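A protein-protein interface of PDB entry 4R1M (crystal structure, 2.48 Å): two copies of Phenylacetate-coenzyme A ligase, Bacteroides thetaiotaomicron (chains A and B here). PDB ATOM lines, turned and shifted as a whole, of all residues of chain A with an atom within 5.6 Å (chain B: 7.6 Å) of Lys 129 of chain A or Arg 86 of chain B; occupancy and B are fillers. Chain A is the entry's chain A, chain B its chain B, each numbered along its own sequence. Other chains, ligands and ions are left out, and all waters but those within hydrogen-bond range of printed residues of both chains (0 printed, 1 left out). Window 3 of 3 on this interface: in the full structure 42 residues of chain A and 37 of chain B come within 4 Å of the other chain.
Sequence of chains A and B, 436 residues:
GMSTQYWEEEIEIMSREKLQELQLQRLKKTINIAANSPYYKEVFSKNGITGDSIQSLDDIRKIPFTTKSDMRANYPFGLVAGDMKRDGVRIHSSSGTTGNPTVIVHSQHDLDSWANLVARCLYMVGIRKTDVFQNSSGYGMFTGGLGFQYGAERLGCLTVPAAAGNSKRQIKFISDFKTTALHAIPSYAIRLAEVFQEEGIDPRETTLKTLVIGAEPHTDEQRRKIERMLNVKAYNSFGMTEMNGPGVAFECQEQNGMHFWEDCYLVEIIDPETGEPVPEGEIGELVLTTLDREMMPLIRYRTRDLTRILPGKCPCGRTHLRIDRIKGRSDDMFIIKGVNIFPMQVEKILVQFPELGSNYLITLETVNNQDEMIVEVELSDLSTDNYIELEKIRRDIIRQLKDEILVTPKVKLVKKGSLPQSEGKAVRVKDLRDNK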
ATOM      1  N   ILE A 127      21.982 -39.762 -25.681  1.00  0.00           N
ATOM      2  CA  ILE A 127      22.317 -38.566 -26.437  1.00  0.00           C
ATOM      3  C   ILE A 127      21.261 -37.509 -26.090  1.00  0.00           C
ATOM      4  O   ILE A 127      20.080 -37.836 -25.963  1.00  0.00           O
ATOM      5  CB  ILE A 127      22.426 -38.889 -27.949  1.00  0.00           C
ATOM      6  CG1 ILE A 127      23.608 -39.880 -28.189  1.00  0.00           C
ATOM      7  CG2 ILE A 127      22.592 -37.603 -28.785  1.00  0.00           C
ATOM      8  CD1 ILE A 127      23.650 -40.515 -29.579  1.00  0.00           C
ATOM      9  N   ARG A 128      21.727 -36.260 -25.845  1.00  0.00           N
ATOM     10  CA  ARG A 128      20.918 -35.097 -25.464  1.00  0.00           C
ATOM     11  C   ARG A 128      21.187 -33.934 -26.426  1.00  0.00           C
ATOM     12  O   ARG A 128      22.037 -34.062 -27.318  1.00  0.00           O
ATOM     13  CB  ARG A 128      21.212 -34.702 -24.008  1.00  0.00           C
ATOM     14  CG  ARG A 128      20.829 -35.797 -22.992  1.00  0.00           C
ATOM     15  CD  ARG A 128      19.332 -36.101 -22.951  1.00  0.00           C
ATOM     16  NE  ARG A 128      19.005 -37.135 -21.966  1.00  0.00           N
ATOM     17  CZ  ARG A 128      18.849 -38.430 -22.236  1.00  0.00           C
ATOM     18  NH1 ARG A 128      18.945 -38.874 -23.485  1.00  0.00           N
ATOM     19  NH2 ARG A 128      18.570 -39.285 -21.263  1.00  0.00           N
ATOM     20  N   LYS A 129      20.426 -32.817 -26.298  1.00  0.00           N
ATOM     21  CA  LYS A 129      20.585 -31.672 -27.208  1.00  0.00           C
ATOM     22  C   LYS A 129      21.982 -31.015 -27.028  1.00  0.00           C
ATOM     23  O   LYS A 129      22.459 -30.356 -27.948  1.00  0.00           O
ATOM     24  CB  LYS A 129      19.464 -30.636 -27.004  1.00  0.00           C
ATOM     25  CG  LYS A 129      19.425 -29.976 -25.617  1.00  0.00           C
ATOM     26  CD  LYS A 129      18.353 -28.883 -25.567  1.00  0.00           C
ATOM     27  CE  LYS A 129      18.611 -27.898 -24.466  1.00  0.00           C
ATOM     28  NZ  LYS A 129      17.635 -26.785 -24.508  1.00  0.00           N
ATOM     29  N   THR A 130      22.642 -31.237 -25.865  1.00  0.00           N
ATOM     30  CA  THR A 130      23.968 -30.677 -25.557  1.00  0.00           C
ATOM     31  C   THR A 130      25.085 -31.448 -26.266  1.00  0.00           C
ATOM     32  O   THR A 130      26.260 -31.068 -26.188  1.00  0.00           O
ATOM     33  CB  THR A 130      24.215 -30.684 -24.054  1.00  0.00           C
ATOM     34  OG1 THR A 130      24.049 -32.017 -23.564  1.00  0.00           O
ATOM     35  CG2 THR A 130      23.303 -29.728 -23.322  1.00  0.00           C
ATOM     36  N   ASP A 131      24.731 -32.548 -26.927  1.00  0.00           N
ATOM     37  CA  ASP A 131      25.712 -33.336 -27.630  1.00  0.00           C
ATOM     38  C   ASP A 131      26.004 -32.713 -29.002  1.00  0.00           C
ATOM     39  O   ASP A 131      25.195 -31.951 -29.542  1.00  0.00           O
ATOM     40  CB  ASP A 131      25.243 -34.797 -27.756  1.00  0.00           C
ATOM     41  CG  ASP A 131      25.516 -35.595 -26.477  1.00  0.00           C
ATOM     42  OD1 ASP A 131      26.703 -35.760 -26.129  1.00  0.00           O
ATOM     43  OD2 ASP A 131      24.533 -36.054 -25.822  1.00  0.00           O
ATOM     44  N   LEU A 155      15.912 -34.126 -32.007  1.00  0.00           N
ATOM     45  CA  LEU A 155      16.369 -34.278 -30.629  1.00  0.00           C
ATOM     46  C   LEU A 155      16.948 -32.932 -30.120  1.00  0.00           C
ATOM     47  O   LEU A 155      16.699 -32.567 -28.963  1.00  0.00           O
ATOM     48  CB  LEU A 155      17.404 -35.413 -30.526  1.00  0.00           C
ATOM     49  CG  LEU A 155      17.740 -35.920 -29.130  1.00  0.00           C
ATOM     50  CD1 LEU A 155      18.270 -37.303 -29.185  1.00  0.00           C
ATOM     51  CD2 LEU A 155      18.757 -35.070 -28.478  1.00  0.00           C
ATOM     52  N   GLY A 156      17.682 -32.222 -30.998  1.00  0.00           N
ATOM     53  CA  GLY A 156      18.288 -30.929 -30.699  1.00  0.00           C
ATOM     54  C   GLY A 156      19.809 -30.878 -30.685  1.00  0.00           C
ATOM     55  O   GLY A 156      20.374 -29.830 -30.354  1.00  0.00           O
ATOM     56  N   CYS A 157      20.499 -31.988 -31.054  1.00  0.00           N
ATOM     57  CA  CYS A 157      21.961 -32.023 -31.090  1.00  0.00           C
ATOM     58  C   CYS A 157      22.527 -30.922 -31.970  1.00  0.00           C
ATOM     59  O   CYS A 157      21.908 -30.558 -32.974  1.00  0.00           O
ATOM     60  CB  CYS A 157      22.471 -33.363 -31.593  1.00  0.00           C
ATOM     61  SG  CYS A 157      21.768 -34.800 -30.782  1.00  0.00           S
ATOM     62  N   LEU A 158      23.762 -30.475 -31.654  1.00  0.00           N
ATOM     63  CA  LEU A 158      24.512 -29.617 -32.544  1.00  0.00           C
ATOM     64  C   LEU A 158      25.095 -30.572 -33.600  1.00  0.00           C
ATOM     65  O   LEU A 158      26.009 -31.330 -33.290  1.00  0.00           O
ATOM     66  CB  LEU A 158      25.542 -28.793 -31.783  1.00  0.00           C
ATOM     67  CG  LEU A 158      26.499 -27.954 -32.642  1.00  0.00           C
ATOM     68  CD1 LEU A 158      25.750 -26.926 -33.465  1.00  0.00           C
ATOM     69  CD2 LEU A 158      27.556 -27.319 -31.797  1.00  0.00           C
ATOM     70  N   GLY B  82      25.231 -16.661 -29.649  1.00  0.00           N
ATOM     71  CA  GLY B  82      24.234 -17.369 -28.851  1.00  0.00           C
ATOM     72  C   GLY B  82      24.799 -18.428 -27.920  1.00  0.00           C
ATOM     73  O   GLY B  82      26.016 -18.512 -27.719  1.00  0.00           O
ATOM     74  N   ASP B  83      23.901 -19.236 -27.315  1.00  0.00           N
ATOM     75  CA  ASP B  83      24.280 -20.337 -26.430  1.00  0.00           C
ATOM     76  C   ASP B  83      24.357 -21.591 -27.292  1.00  0.00           C
ATOM     77  O   ASP B  83      23.353 -22.253 -27.533  1.00  0.00           O
ATOM     78  CB  ASP B  83      23.304 -20.485 -25.243  1.00  0.00           C
ATOM     79  CG  ASP B  83      23.796 -21.384 -24.122  1.00  0.00           C
ATOM     80  OD1 ASP B  83      24.741 -22.182 -24.355  1.00  0.00           O
ATOM     81  OD2 ASP B  83      23.243 -21.292 -23.005  1.00  0.00           O
ATOM     82  N   MET B  84      25.542 -21.877 -27.811  1.00  0.00           N
ATOM     83  CA  MET B  84      25.738 -22.974 -28.742  1.00  0.00           C
ATOM     84  C   MET B  84      25.398 -24.327 -28.098  1.00  0.00           C
ATOM     85  O   MET B  84      24.734 -25.136 -28.747  1.00  0.00           O
ATOM     86  CB  MET B  84      27.176 -22.960 -29.247  1.00  0.00           C
ATOM     87  CG  MET B  84      27.410 -23.891 -30.415  1.00  0.00           C
ATOM     88  SD  MET B  84      29.192 -23.730 -31.153  1.00  0.00           S
ATOM     89  CE  MET B  84      30.273 -24.184 -29.668  1.00  0.00           C
ATOM     90  N   LYS B  85      25.791 -24.549 -26.827  1.00  0.00           N
ATOM     91  CA  LYS B  85      25.543 -25.823 -26.137  1.00  0.00           C
ATOM     92  C   LYS B  85      24.040 -26.046 -25.905  1.00  0.00           C
ATOM     93  O   LYS B  85      23.549 -27.175 -26.046  1.00  0.00           O
ATOM     94  CB  LYS B  85      26.300 -25.880 -24.795  1.00  0.00           C
ATOM     95  CG  LYS B  85      26.427 -27.316 -24.283  1.00  0.00           C
ATOM     96  CD  LYS B  85      27.252 -27.531 -23.028  1.00  0.00           C
ATOM     97  CE  LYS B  85      27.411 -29.035 -22.820  1.00  0.00           C
ATOM     98  NZ  LYS B  85      28.161 -29.414 -21.594  1.00  0.00           N
ATOM     99  N   ARG B  86      23.324 -24.958 -25.575  1.00  0.00           N
ATOM    100  CA  ARG B  86      21.895 -24.974 -25.296  1.00  0.00           C
ATOM    101  C   ARG B  86      20.994 -24.968 -26.552  1.00  0.00           C
ATOM    102  O   ARG B  86      19.924 -25.572 -26.499  1.00  0.00           O
ATOM    103  CB  ARG B  86      21.550 -23.724 -24.476  1.00  0.00           C
ATOM    104  CG  ARG B  86      20.221 -23.752 -23.763  1.00  0.00           C
ATOM    105  CD  ARG B  86      19.770 -22.366 -23.355  1.00  0.00           C
ATOM    106  NE  ARG B  86      18.583 -22.431 -22.496  1.00  0.00           N
ATOM    107  CZ  ARG B  86      17.327 -22.502 -22.932  1.00  0.00           C
ATOM    108  NH1 ARG B  86      17.069 -22.513 -24.237  1.00  0.00           N
ATOM    109  NH2 ARG B  86      16.320 -22.560 -22.067  1.00  0.00           N
ATOM    110  N   ASP B  87      21.379 -24.232 -27.637  1.00  0.00           N
ATOM    111  CA  ASP B  87      20.521 -23.954 -28.788  1.00  0.00           C
ATOM    112  C   ASP B  87      21.131 -24.233 -30.180  1.00  0.00           C
ATOM    113  O   ASP B  87      20.388 -24.158 -31.161  1.00  0.00           O
ATOM    114  CB  ASP B  87      20.156 -22.463 -28.742  1.00  0.00           C
ATOM    115  CG  ASP B  87      19.430 -22.031 -27.481  1.00  0.00           C
ATOM    116  OD1 ASP B  87      18.622 -22.832 -26.955  1.00  0.00           O
ATOM    117  OD2 ASP B  87      19.614 -20.866 -27.061  1.00  0.00           O
ATOM    118  N   GLY B  88      22.424 -24.541 -30.274  1.00  0.00           N
ATOM    119  CA  GLY B  88      23.049 -24.833 -31.571  1.00  0.00           C
ATOM    120  C   GLY B  88      22.522 -26.132 -32.157  1.00  0.00           C
ATOM    121  O   GLY B  88      22.431 -27.121 -31.424  1.00  0.00           O
ATOM    122  N   VAL B  89      22.105 -26.144 -33.458  1.00  0.00           N
ATOM    123  CA  VAL B  89      21.554 -27.392 -34.028  1.00  0.00           C
ATOM    124  C   VAL B  89      22.331 -27.810 -35.299  1.00  0.00           C
ATOM    125  O   VAL B  89      22.207 -28.960 -35.709  1.00  0.00           O
ATOM    126  CB  VAL B  89      20.026 -27.360 -34.319  1.00  0.00           C
ATOM    127  CG1 VAL B  89      19.237 -27.008 -33.068  1.00  0.00           C
ATOM    128  CG2 VAL B  89      19.698 -26.408 -35.433  1.00  0.00           C
ATOM    129  N   MET B 295      22.263 -17.161 -33.790  1.00  0.00           N
ATOM    130  CA  MET B 295      23.377 -17.906 -33.188  1.00  0.00           C
ATOM    131  C   MET B 295      24.731 -17.242 -33.506  1.00  0.00           C
ATOM    132  O   MET B 295      25.544 -17.028 -32.591  1.00  0.00           O
ATOM    133  CB  MET B 295      23.376 -19.372 -33.669  1.00  0.00           C
ATOM    134  CG  MET B 295      24.504 -20.234 -33.078  1.00  0.00           C
ATOM    135  SD  MET B 295      24.594 -20.310 -31.141  1.00  0.00           S
ATOM    136  CE  MET B 295      22.854 -21.086 -30.804  1.00  0.00           C
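Among the printed residues, merely in contact across the chains: Leu 158 of chain A with Gly 88 of chain B, Thr 130 of chain A with Lys 85 of chain B, Gly 156 of chain A with Gly 88 of chain B, Leu 158 of chain A with Met 84 of chain B, Leu 158 of chain A with Val 89 of chain B, Cys 157 of chain A with Gly 88 of chain B and Lys 129 of chain A with Lys 85 of chain B.
No position is printed for both chains.
Of the 9 pairs that touch across the chains among the printed residues, none has its exchanged pair printed and touching as well.
Printed residues of chain A that touch a printed residue of chain B: Lys 129, Thr 130, Gly 156, Cys 157 and Leu 158.
Hydrophobic or aromatic side chains of chain A within 4 Å of the printed part of chain B: Leu 158.
Along chain A the printed residues that touch a printed residue of chain B span positions 129 to 158.
Of the 9 printed residues of chain B, 5 touch a printed residue of chain A.
Hydrophobic or aromatic side chains of chain B that line the printed part of chain A: Met 84 and Val 89.
Among the printed residues, no Asp or Glu carboxylate lies within 4 Å of a Lys or Arg side-chain nitrogen of the other chain.
The backbone carbonyl oxygen (O) of Arg 128 of chain A sits at hydrogen-bond distance from the side-chain sulfur (SG) of Cys 157 of chain A (3.6 Å).
The guanidinium group (NH1) of Arg 86 of chain B lies within salt-bridge range of the side-chain carboxylate (OD1) of Asp 87 of chain B (3.1 Å).
OD1 of Asp 83 of chain B sits at hydrogen-bond distance from N of Arg 86 of chain B (3.3 Å).
O of Asp 131 of chain A is in hydrogen-bond range of N of Leu 158 of chain A (2.9 Å).
Of chain B, only Lys 85 and Arg 86 come within 4 Å of Lys 129 of chain A.
Arg 86 of chain B touches one residue of chain A.
Of the printed residues of chain B, Cys 157 of chain A touches Gly 88 and Val 89.
Printed residues of chain A within 4 Å of Met 84 of chain B: Leu 158 (3.7 Å).
Of the printed residues of chain A, Gly 88 of chain B touches Gly 156 (3.6 Å), Cys 157 (3.8 Å) and Leu 158 (3.4 Å).
Of the printed residues of chain B, Gly 156 of chain A touches Gly 88.
Arg 128 of chain A touches none of the printed residues of chain B.
The nearest printed residue of chain A that does not touch Gly 88 of chain B is Lys 129 of chain A (4.7 Å).
The side-chain amino group (NZ) of Lys 129 of chain A sits at hydrogen-bond distance from the backbone carbonyl oxygen (O) of Arg 86 of chain B (3.3 Å).
O of Cys 157 of chain A sits close to O of Val 89 of chain B (3.2 Å).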
